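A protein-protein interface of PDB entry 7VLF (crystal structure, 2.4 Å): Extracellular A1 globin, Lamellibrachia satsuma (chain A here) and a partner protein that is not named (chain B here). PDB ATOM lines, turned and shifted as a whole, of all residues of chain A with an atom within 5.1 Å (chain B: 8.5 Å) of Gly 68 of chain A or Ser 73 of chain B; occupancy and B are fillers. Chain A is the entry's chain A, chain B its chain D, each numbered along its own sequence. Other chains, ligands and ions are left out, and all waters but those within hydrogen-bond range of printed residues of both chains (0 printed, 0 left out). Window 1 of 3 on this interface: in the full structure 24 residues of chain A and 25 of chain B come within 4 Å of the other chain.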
ATOM      1  N   TYR A  18      -2.286  29.909  -6.136  1.00  0.00           N
ATOM      2  CA  TYR A  18      -1.734  29.522  -7.432  1.00  0.00           C
ATOM      3  C   TYR A  18      -2.799  29.556  -8.522  1.00  0.00           C
ATOM      4  O   TYR A  18      -2.544  30.046  -9.629  1.00  0.00           O
ATOM      5  CB  TYR A  18      -1.105  28.132  -7.342  1.00  0.00           C
ATOM      6  CG  TYR A  18      -0.227  27.777  -8.520  1.00  0.00           C
ATOM      7  CD1 TYR A  18       0.316  28.768  -9.328  1.00  0.00           C
ATOM      8  CD2 TYR A  18       0.050  26.451  -8.831  1.00  0.00           C
ATOM      9  CE1 TYR A  18       1.112  28.453 -10.407  1.00  0.00           C
ATOM     10  CE2 TYR A  18       0.848  26.125  -9.911  1.00  0.00           C
ATOM     11  CZ  TYR A  18       1.377  27.131 -10.695  1.00  0.00           C
ATOM     12  OH  TYR A  18       2.173  26.820 -11.773  1.00  0.00           O
ATOM     13  N   ILE A  63       9.345  30.211 -16.466  1.00  0.00           N
ATOM     14  CA  ILE A  63       8.441  30.473 -15.351  1.00  0.00           C
ATOM     15  C   ILE A  63       7.579  29.250 -15.070  1.00  0.00           C
ATOM     16  O   ILE A  63       7.415  28.835 -13.916  1.00  0.00           O
ATOM     17  CB  ILE A  63       7.576  31.715 -15.641  1.00  0.00           C
ATOM     18  CG1 ILE A  63       8.425  32.984 -15.591  1.00  0.00           C
ATOM     19  CG2 ILE A  63       6.415  31.806 -14.663  1.00  0.00           C
ATOM     20  CD1 ILE A  63       7.633  34.243 -15.841  1.00  0.00           C
ATOM     21  N   ALA A  64       7.031  28.643 -16.124  1.00  0.00           N
ATOM     22  CA  ALA A  64       6.118  27.521 -15.939  1.00  0.00           C
ATOM     23  C   ALA A  64       6.810  26.338 -15.275  1.00  0.00           C
ATOM     24  O   ALA A  64       6.234  25.682 -14.399  1.00  0.00           O
ATOM     25  CB  ALA A  64       5.524  27.101 -17.284  1.00  0.00           C
ATOM     26  N   ARG A  65       8.047  26.047 -15.683  1.00  0.00           N
ATOM     27  CA  ARG A  65       8.749  24.892 -15.133  1.00  0.00           C
ATOM     28  C   ARG A  65       9.161  25.125 -13.685  1.00  0.00           C
ATOM     29  O   ARG A  65       9.116  24.199 -12.868  1.00  0.00           O
ATOM     30  CB  ARG A  65       9.970  24.557 -15.990  1.00  0.00           C
ATOM     31  CG  ARG A  65       9.639  23.853 -17.296  1.00  0.00           C
ATOM     32  CD  ARG A  65      10.899  23.411 -18.024  1.00  0.00           C
ATOM     33  NE  ARG A  65      11.744  24.543 -18.388  1.00  0.00           N
ATOM     34  CZ  ARG A  65      11.678  25.178 -19.554  1.00  0.00           C
ATOM     35  NH1 ARG A  65      10.807  24.789 -20.475  1.00  0.00           N
ATOM     36  NH2 ARG A  65      12.484  26.201 -19.800  1.00  0.00           N
ATOM     37  N   VAL A  66       9.561  26.351 -13.346  1.00  0.00           N
ATOM     38  CA  VAL A  66      10.034  26.630 -11.993  1.00  0.00           C
ATOM     39  C   VAL A  66       8.882  26.557 -10.997  1.00  0.00           C
ATOM     40  O   VAL A  66       8.928  25.795 -10.024  1.00  0.00           O
ATOM     41  CB  VAL A  66      10.741  27.994 -11.937  1.00  0.00           C
ATOM     42  CG1 VAL A  66      10.970  28.405 -10.495  1.00  0.00           C
ATOM     43  CG2 VAL A  66      12.061  27.928 -12.681  1.00  0.00           C
ATOM     44  N   ILE A  67       7.837  27.356 -11.220  1.00  0.00           N
ATOM     45  CA  ILE A  67       6.699  27.351 -10.305  1.00  0.00           C
ATOM     46  C   ILE A  67       5.955  26.022 -10.373  1.00  0.00           C
ATOM     47  O   ILE A  67       5.380  25.572  -9.372  1.00  0.00           O
ATOM     48  CB  ILE A  67       5.776  28.549 -10.599  1.00  0.00           C
ATOM     49  CG1 ILE A  67       6.458  29.857 -10.196  1.00  0.00           C
ATOM     50  CG2 ILE A  67       4.474  28.427  -9.849  1.00  0.00           C
ATOM     51  CD1 ILE A  67       7.102  30.590 -11.336  1.00  0.00           C
ATOM     52  N   GLY A  68       5.978  25.355 -11.529  1.00  0.00           N
ATOM     53  CA  GLY A  68       5.413  24.019 -11.606  1.00  0.00           C
ATOM     54  C   GLY A  68       6.121  23.038 -10.691  1.00  0.00           C
ATOM     55  O   GLY A  68       5.480  22.233 -10.009  1.00  0.00           O
ATOM     56  N   GLY A  69       7.454  23.097 -10.656  1.00  0.00           N
ATOM     57  CA  GLY A  69       8.195  22.268  -9.721  1.00  0.00           C
ATOM     58  C   GLY A  69       7.964  22.681  -8.281  1.00  0.00           C
ATOM     59  O   GLY A  69       7.917  21.835  -7.383  1.00  0.00           O
ATOM     60  N   LEU A  70       7.821  23.986  -8.038  1.00  0.00           N
ATOM     61  CA  LEU A  70       7.445  24.450  -6.708  1.00  0.00           C
ATOM     62  C   LEU A  70       6.066  23.933  -6.325  1.00  0.00           C
ATOM     63  O   LEU A  70       5.820  23.596  -5.162  1.00  0.00           O
ATOM     64  CB  LEU A  70       7.488  25.978  -6.654  1.00  0.00           C
ATOM     65  CG  LEU A  70       7.200  26.617  -5.295  1.00  0.00           C
ATOM     66  CD1 LEU A  70       8.086  26.007  -4.222  1.00  0.00           C
ATOM     67  CD2 LEU A  70       7.398  28.124  -5.358  1.00  0.00           C
ATOM     68  N   ASP A  71       5.155  23.845  -7.297  1.00  0.00           N
ATOM     69  CA  ASP A  71       3.845  23.261  -7.028  1.00  0.00           C
ATOM     70  C   ASP A  71       3.964  21.784  -6.676  1.00  0.00           C
ATOM     71  O   ASP A  71       3.271  21.295  -5.776  1.00  0.00           O
ATOM     72  CB  ASP A  71       2.924  23.464  -8.234  1.00  0.00           C
ATOM     73  CG  ASP A  71       1.639  22.660  -8.134  1.00  0.00           C
ATOM     74  OD1 ASP A  71       1.635  21.478  -8.542  1.00  0.00           O
ATOM     75  OD2 ASP A  71       0.636  23.210  -7.639  1.00  0.00           O
ATOM     76  N   ARG A  72       4.843  21.056  -7.369  1.00  0.00           N
ATOM     77  CA  ARG A  72       4.970  19.626  -7.110  1.00  0.00           C
ATOM     78  C   ARG A  72       5.737  19.352  -5.824  1.00  0.00           C
ATOM     79  O   ARG A  72       5.510  18.323  -5.180  1.00  0.00           O
ATOM     80  CB  ARG A  72       5.638  18.931  -8.297  1.00  0.00           C
ATOM     81  CG  ARG A  72       7.157  18.930  -8.290  1.00  0.00           C
ATOM     82  CD  ARG A  72       7.700  18.051  -9.411  1.00  0.00           C
ATOM     83  NE  ARG A  72       9.137  17.818  -9.292  1.00  0.00           N
ATOM     84  CZ  ARG A  72      10.061  18.428 -10.029  1.00  0.00           C
ATOM     85  NH1 ARG A  72       9.704  19.313 -10.948  1.00  0.00           N
ATOM     86  NH2 ARG A  72      11.346  18.151  -9.850  1.00  0.00           N
ATOM     87  N   TRP B  16      -9.233  18.286 -15.560  1.00  0.00           N
ATOM     88  CA  TRP B  16      -7.931  17.916 -15.017  1.00  0.00           C
ATOM     89  C   TRP B  16      -7.735  18.484 -13.617  1.00  0.00           C
ATOM     90  O   TRP B  16      -7.237  17.789 -12.723  1.00  0.00           O
ATOM     91  CB  TRP B  16      -6.820  18.393 -15.952  1.00  0.00           C
ATOM     92  CG  TRP B  16      -5.452  18.310 -15.358  1.00  0.00           C
ATOM     93  CD1 TRP B  16      -4.628  19.352 -15.048  1.00  0.00           C
ATOM     94  CD2 TRP B  16      -4.743  17.118 -14.996  1.00  0.00           C
ATOM     95  NE1 TRP B  16      -3.451  18.884 -14.519  1.00  0.00           N
ATOM     96  CE2 TRP B  16      -3.496  17.516 -14.476  1.00  0.00           C
ATOM     97  CE3 TRP B  16      -5.042  15.753 -15.062  1.00  0.00           C
ATOM     98  CZ2 TRP B  16      -2.547  16.600 -14.028  1.00  0.00           C
ATOM     99  CZ3 TRP B  16      -4.099  14.846 -14.612  1.00  0.00           C
ATOM    100  CH2 TRP B  16      -2.868  15.273 -14.101  1.00  0.00           C
ATOM    101  N   TYR B  20      -6.561  16.839 -10.001  1.00  0.00           N
ATOM    102  CA  TYR B  20      -5.150  17.150  -9.785  1.00  0.00           C
ATOM    103  C   TYR B  20      -5.003  18.629  -9.460  1.00  0.00           C
ATOM    104  O   TYR B  20      -5.113  19.479 -10.348  1.00  0.00           O
ATOM    105  CB  TYR B  20      -4.309  16.775 -11.009  1.00  0.00           C
ATOM    106  CG  TYR B  20      -2.812  16.831 -10.773  1.00  0.00           C
ATOM    107  CD1 TYR B  20      -2.134  18.045 -10.759  1.00  0.00           C
ATOM    108  CD2 TYR B  20      -2.077  15.670 -10.575  1.00  0.00           C
ATOM    109  CE1 TYR B  20      -0.767  18.100 -10.542  1.00  0.00           C
ATOM    110  CE2 TYR B  20      -0.710  15.715 -10.362  1.00  0.00           C
ATOM    111  CZ  TYR B  20      -0.059  16.934 -10.348  1.00  0.00           C
ATOM    112  OH  TYR B  20       1.301  16.985 -10.136  1.00  0.00           O
ATOM    113  N   ALA B  22      -2.853  21.206  -6.097  1.00  0.00           N
ATOM    114  CA  ALA B  22      -1.788  21.151  -5.105  1.00  0.00           C
ATOM    115  C   ALA B  22      -2.281  20.662  -3.750  1.00  0.00           C
ATOM    116  O   ALA B  22      -1.543  19.967  -3.043  1.00  0.00           O
ATOM    117  CB  ALA B  22      -1.131  22.524  -4.965  1.00  0.00           C
ATOM    118  N   ARG B  29      -1.812  11.069  -4.807  1.00  0.00           N
ATOM    119  CA  ARG B  29      -0.881  11.247  -5.915  1.00  0.00           C
ATOM    120  C   ARG B  29      -0.082   9.973  -6.188  1.00  0.00           C
ATOM    121  O   ARG B  29       0.370   9.765  -7.318  1.00  0.00           O
ATOM    122  CB  ARG B  29       0.055  12.423  -5.628  1.00  0.00           C
ATOM    123  CG  ARG B  29      -0.583  13.555  -4.843  1.00  0.00           C
ATOM    124  CD  ARG B  29       0.359  14.738  -4.737  1.00  0.00           C
ATOM    125  NE  ARG B  29       0.330  15.562  -5.940  1.00  0.00           N
ATOM    126  CZ  ARG B  29      -0.455  16.624  -6.090  1.00  0.00           C
ATOM    127  NH1 ARG B  29      -1.268  16.985  -5.107  1.00  0.00           N
ATOM    128  NH2 ARG B  29      -0.426  17.328  -7.212  1.00  0.00           N
ATOM    129  N   ALA B  66       8.702  10.258  -6.336  1.00  0.00           N
ATOM    130  CA  ALA B  66       9.061  11.602  -6.777  1.00  0.00           C
ATOM    131  C   ALA B  66       9.177  11.688  -8.292  1.00  0.00           C
ATOM    132  O   ALA B  66       8.990  12.767  -8.866  1.00  0.00           O
ATOM    133  CB  ALA B  66      10.369  12.055  -6.124  1.00  0.00           C
ATOM    134  N   HIS B  67       9.481  10.571  -8.955  1.00  0.00           N
ATOM    135  CA  HIS B  67       9.558  10.579 -10.411  1.00  0.00           C
ATOM    136  C   HIS B  67       8.177  10.708 -11.038  1.00  0.00           C
ATOM    137  O   HIS B  67       7.990  11.473 -11.991  1.00  0.00           O
ATOM    138  CB  HIS B  67      10.247   9.311 -10.907  1.00  0.00           C
ATOM    139  CG  HIS B  67      10.118   9.101 -12.381  1.00  0.00           C
ATOM    140  ND1 HIS B  67      10.803   9.862 -13.304  1.00  0.00           N
ATOM    141  CD2 HIS B  67       9.372   8.225 -13.094  1.00  0.00           C
ATOM    142  CE1 HIS B  67      10.491   9.457 -14.522  1.00  0.00           C
ATOM    143  NE2 HIS B  67       9.624   8.465 -14.423  1.00  0.00           N
ATOM    144  N   THR B  68       7.198   9.960 -10.524  1.00  0.00           N
ATOM    145  CA  THR B  68       5.850  10.036 -11.074  1.00  0.00           C
ATOM    146  C   THR B  68       5.254  11.427 -10.909  1.00  0.00           C
ATOM    147  O   THR B  68       4.458  11.863 -11.749  1.00  0.00           O
ATOM    148  CB  THR B  68       4.949   8.993 -10.413  1.00  0.00           C
ATOM    149  OG1 THR B  68       4.915   9.213  -8.998  1.00  0.00           O
ATOM    150  CG2 THR B  68       5.474   7.593 -10.689  1.00  0.00           C
ATOM    151  N   VAL B  69       5.628  12.140  -9.846  1.00  0.00           N
ATOM    152  CA  VAL B  69       5.136  13.500  -9.661  1.00  0.00           C
ATOM    153  C   VAL B  69       5.762  14.436 -10.683  1.00  0.00           C
ATOM    154  O   VAL B  69       5.085  15.308 -11.242  1.00  0.00           O
ATOM    155  CB  VAL B  69       5.398  13.970  -8.220  1.00  0.00           C
ATOM    156  CG1 VAL B  69       5.326  15.476  -8.139  1.00  0.00           C
ATOM    157  CG2 VAL B  69       4.378  13.364  -7.293  1.00  0.00           C
ATOM    158  N   ARG B  70       7.060  14.268 -10.949  1.00  0.00           N
ATOM    159  CA  ARG B  70       7.716  15.052 -11.989  1.00  0.00           C
ATOM    160  C   ARG B  70       6.978  14.922 -13.313  1.00  0.00           C
ATOM    161  O   ARG B  70       6.712  15.918 -13.994  1.00  0.00           O
ATOM    162  CB  ARG B  70       9.174  14.610 -12.141  1.00  0.00           C
ATOM    163  CG  ARG B  70      10.078  14.982 -10.981  1.00  0.00           C
ATOM    164  CD  ARG B  70      11.445  14.328 -11.126  1.00  0.00           C
ATOM    165  NE  ARG B  70      11.681  13.330 -10.087  1.00  0.00           N
ATOM    166  CZ  ARG B  70      12.624  12.394 -10.143  1.00  0.00           C
ATOM    167  NH1 ARG B  70      13.423  12.313 -11.199  1.00  0.00           N
ATOM    168  NH2 ARG B  70      12.760  11.530  -9.146  1.00  0.00           N
ATOM    169  N   VAL B  71       6.621  13.692 -13.683  1.00  0.00           N
ATOM    170  CA  VAL B  71       5.885  13.463 -14.922  1.00  0.00           C
ATOM    171  C   VAL B  71       4.502  14.101 -14.851  1.00  0.00           C
ATOM    172  O   VAL B  71       4.045  14.735 -15.810  1.00  0.00           O
ATOM    173  CB  VAL B  71       5.795  11.955 -15.208  1.00  0.00           C
ATOM    174  CG1 VAL B  71       5.012  11.704 -16.485  1.00  0.00           C
ATOM    175  CG2 VAL B  71       7.189  11.351 -15.291  1.00  0.00           C
ATOM    176  N   LEU B  72       3.809  13.949 -13.718  1.00  0.00           N
ATOM    177  CA  LEU B  72       2.471  14.519 -13.597  1.00  0.00           C
ATOM    178  C   LEU B  72       2.520  16.038 -13.494  1.00  0.00           C
ATOM    179  O   LEU B  72       1.635  16.726 -14.015  1.00  0.00           O
ATOM    180  CB  LEU B  72       1.746  13.922 -12.392  1.00  0.00           C
ATOM    181  CG  LEU B  72       1.360  12.448 -12.527  1.00  0.00           C
ATOM    182  CD1 LEU B  72       0.576  11.960 -11.315  1.00  0.00           C
ATOM    183  CD2 LEU B  72       0.570  12.231 -13.806  1.00  0.00           C
ATOM    184  N   SER B  73       3.535  16.580 -12.817  1.00  0.00           N
ATOM    185  CA  SER B  73       3.685  18.030 -12.765  1.00  0.00           C
ATOM    186  C   SER B  73       3.953  18.600 -14.152  1.00  0.00           C
ATOM    187  O   SER B  73       3.451  19.676 -14.497  1.00  0.00           O
ATOM    188  CB  SER B  73       4.808  18.412 -11.803  1.00  0.00           C
ATOM    189  OG  SER B  73       4.965  19.817 -11.745  1.00  0.00           O
ATOM    190  N   GLY B  74       4.746  17.894 -14.959  1.00  0.00           N
ATOM    191  CA  GLY B  74       4.949  18.320 -16.333  1.00  0.00           C
ATOM    192  C   GLY B  74       3.688  18.192 -17.164  1.00  0.00           C
ATOM    193  O   GLY B  74       3.410  19.034 -18.022  1.00  0.00           O
ATOM    194  N   LEU B  75       2.909  17.134 -16.924  1.00  0.00           N
ATOM    195  CA  LEU B  75       1.615  17.003 -17.586  1.00  0.00           C
ATOM    196  C   LEU B  75       0.634  18.054 -17.085  1.00  0.00           C
ATOM    197  O   LEU B  75      -0.102  18.653 -17.878  1.00  0.00           O
ATOM    198  CB  LEU B  75       1.057  15.597 -17.367  1.00  0.00           C
ATOM    199  CG  LEU B  75      -0.404  15.365 -17.755  1.00  0.00           C
ATOM    200  CD1 LEU B  75      -0.617  15.608 -19.241  1.00  0.00           C
ATOM    201  CD2 LEU B  75      -0.843  13.961 -17.367  1.00  0.00           C
ATOM    202  N   ASP B  76       0.608  18.290 -15.771  1.00  0.00           N
ATOM    203  CA  ASP B  76      -0.247  19.340 -15.226  1.00  0.00           C
ATOM    204  C   ASP B  76       0.160  20.710 -15.743  1.00  0.00           C
ATOM    205  O   ASP B  76      -0.691  21.593 -15.906  1.00  0.00           O
ATOM    206  CB  ASP B  76      -0.204  19.302 -13.699  1.00  0.00           C
ATOM    207  CG  ASP B  76      -0.806  20.538 -13.061  1.00  0.00           C
ATOM    208  OD1 ASP B  76      -0.087  21.551 -12.926  1.00  0.00           O
ATOM    209  OD2 ASP B  76      -2.001  20.501 -12.700  1.00  0.00           O
ATOM    210  N   MET B  77       1.451  20.907 -16.005  1.00  0.00           N
ATOM    211  CA  MET B  77       1.906  22.166 -16.581  1.00  0.00           C
ATOM    212  C   MET B  77       1.377  22.344 -17.999  1.00  0.00           C
ATOM    213  O   MET B  77       0.901  23.425 -18.367  1.00  0.00           O
ATOM    214  CB  MET B  77       3.434  22.221 -16.560  1.00  0.00           C
ATOM    215  CG  MET B  77       4.038  23.198 -17.552  1.00  0.00           C
ATOM    216  SD  MET B  77       5.834  23.273 -17.423  1.00  0.00           S
ATOM    217  CE  MET B  77       6.263  21.539 -17.557  1.00  0.00           C
ATOM    218  N   GLY B  78       1.450  21.289 -18.814  1.00  0.00           N
ATOM    219  CA  GLY B  78       1.018  21.401 -20.198  1.00  0.00           C
ATOM    220  C   GLY B  78      -0.477  21.611 -20.340  1.00  0.00           C
ATOM    221  O   GLY B  78      -0.926  22.363 -21.210  1.00  0.00           O
ATOM    222  N   ILE B  79      -1.271  20.960 -19.487  1.00  0.00           N
ATOM    223  CA  ILE B  79      -2.722  21.082 -19.587  1.00  0.00           C
ATOM    224  C   ILE B  79      -3.158  22.506 -19.270  1.00  0.00           C
ATOM    225  O   ILE B  79      -3.949  23.109 -20.003  1.00  0.00           O
ATOM    226  CB  ILE B  79      -3.413  20.061 -18.668  1.00  0.00           C
ATOM    227  CG1 ILE B  79      -3.138  18.642 -19.163  1.00  0.00           C
ATOM    228  CG2 ILE B  79      -4.908  20.335 -18.596  1.00  0.00           C
ATOM    229  CD1 ILE B  79      -3.802  17.567 -18.339  1.00  0.00           C
ATOM    230  N   ASN B  80      -2.642  23.068 -18.177  1.00  0.00           N
ATOM    231  CA  ASN B  80      -3.009  24.422 -17.787  1.00  0.00           C
ATOM    232  C   ASN B  80      -2.463  25.484 -18.730  1.00  0.00           C
ATOM    233  O   ASN B  80      -2.832  26.655 -18.592  1.00  0.00           O
ATOM    234  CB  ASN B  80      -2.531  24.699 -16.363  1.00  0.00           C
ATOM    235  CG  ASN B  80      -3.220  23.819 -15.343  1.00  0.00           C
ATOM    236  OD1 ASN B  80      -4.240  24.197 -14.769  1.00  0.00           O
ATOM    237  ND2 ASN B  80      -2.669  22.634 -15.116  1.00  0.00           N
ATOM    238  N   TYR B  81      -1.600  25.114 -19.676  1.00  0.00           N
ATOM    239  CA  TYR B  81      -1.088  26.044 -20.673  1.00  0.00           C
ATOM    240  C   TYR B  81      -1.636  25.764 -22.066  1.00  0.00           C
ATOM    241  O   TYR B  81      -1.076  26.252 -23.054  1.00  0.00           O
ATOM    242  CB  TYR B  81       0.440  26.010 -20.695  1.00  0.00           C
ATOM    243  CG  TYR B  81       1.094  26.904 -19.668  1.00  0.00           C
ATOM    244  CD1 TYR B  81       1.207  26.506 -18.344  1.00  0.00           C
ATOM    245  CD2 TYR B  81       1.611  28.143 -20.027  1.00  0.00           C
ATOM    246  CE1 TYR B  81       1.811  27.319 -17.404  1.00  0.00           C
ATOM    247  CE2 TYR B  81       2.217  28.963 -19.094  1.00  0.00           C
ATOM    248  CZ  TYR B  81       2.314  28.546 -17.785  1.00  0.00           C
ATOM    249  OH  TYR B  81       2.918  29.358 -16.851  1.00  0.00           O
ATOM    250  N   LEU B  95      10.611  19.470 -23.428  1.00  0.00           N
ATOM    251  CA  LEU B  95      10.446  18.110 -22.931  1.00  0.00           C
ATOM    252  C   LEU B  95      10.850  17.069 -23.967  1.00  0.00           C
ATOM    253  O   LEU B  95      11.308  15.981 -23.596  1.00  0.00           O
ATOM    254  CB  LEU B  95       8.999  17.874 -22.493  1.00  0.00           C
ATOM    255  CG  LEU B  95       8.612  18.424 -21.121  1.00  0.00           C
ATOM    256  CD1 LEU B  95       7.222  17.950 -20.732  1.00  0.00           C
ATOM    257  CD2 LEU B  95       9.636  18.015 -20.072  1.00  0.00           C
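The backbone carbonyl oxygen of Gly 68 of chain A is in hydrogen-bond range of the side-chain hydroxyl of Ser 73 of chain B (3.0 Å).
The backbone carbonyl oxygen (O) of Ala 66 of chain B is in hydrogen-bond range of the guanidinium group (NE) of Arg 70 of chain B, at 3.0 Å.
Of the 21 printed residues of chain B, 6 touch a printed residue of chain A.
Along chain B the printed residues that touch a printed residue of chain A span positions 22 to 81.
Of the 11 printed residues of chain A, 5 touch a printed residue of chain B.
Hydrophobic or aromatic side chains of chain A within 4 Å of the printed part of chain B: Ala 64.
No residue of chain B comes within 4 Å of Gly 69 of chain A.
Leu 70 of chain A touches none of the printed residues of chain B.
Printed residues of chain A within 4 Å of Ala 22 of chain B: Asp 71.
Of the printed residues of chain A, Arg 70 of chain B touches Arg 72 (3.4 Å).
Leu 72 of chain B touches none of the printed residues of chain A.
Of chain A, only Gly 68 (3.0 Å) and Arg 72 (3.6 Å) come within 4 Å of Ser 73 of chain B.
Printed residues of chain A within 4 Å of Met 77 of chain B: Ala 64 (3.8 Å) and Arg 65 (3.9 Å).
The nearest residue of chain B that does not touch Gly 68 of chain A is Met 77 of chain B (5.6 Å).
The nearest residue of chain A that does not touch Ser 73 of chain B is Gly 69 of chain A (4.3 Å).
Ala 64 of chain A touches Met 77 of chain B.
OH of Tyr 81 of chain B touches CB of Ala 64 of chain A (3.5 Å).
CG of Arg 65 of chain A touches SD of Met 77 of chain B (3.9 Å).
OD2 of Asp 71 of chain A touches CB of Ala 22 of chain B (3.3 Å).
Val 69 of chain B touches Arg 72 of chain A.
Arg 70 of chain B touches Arg 72 of chain A (CG to NE, 3.4 Å).
CB of Arg 72 of chain A touches OG of Ser 73 of chain B, 3.6 Å away.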
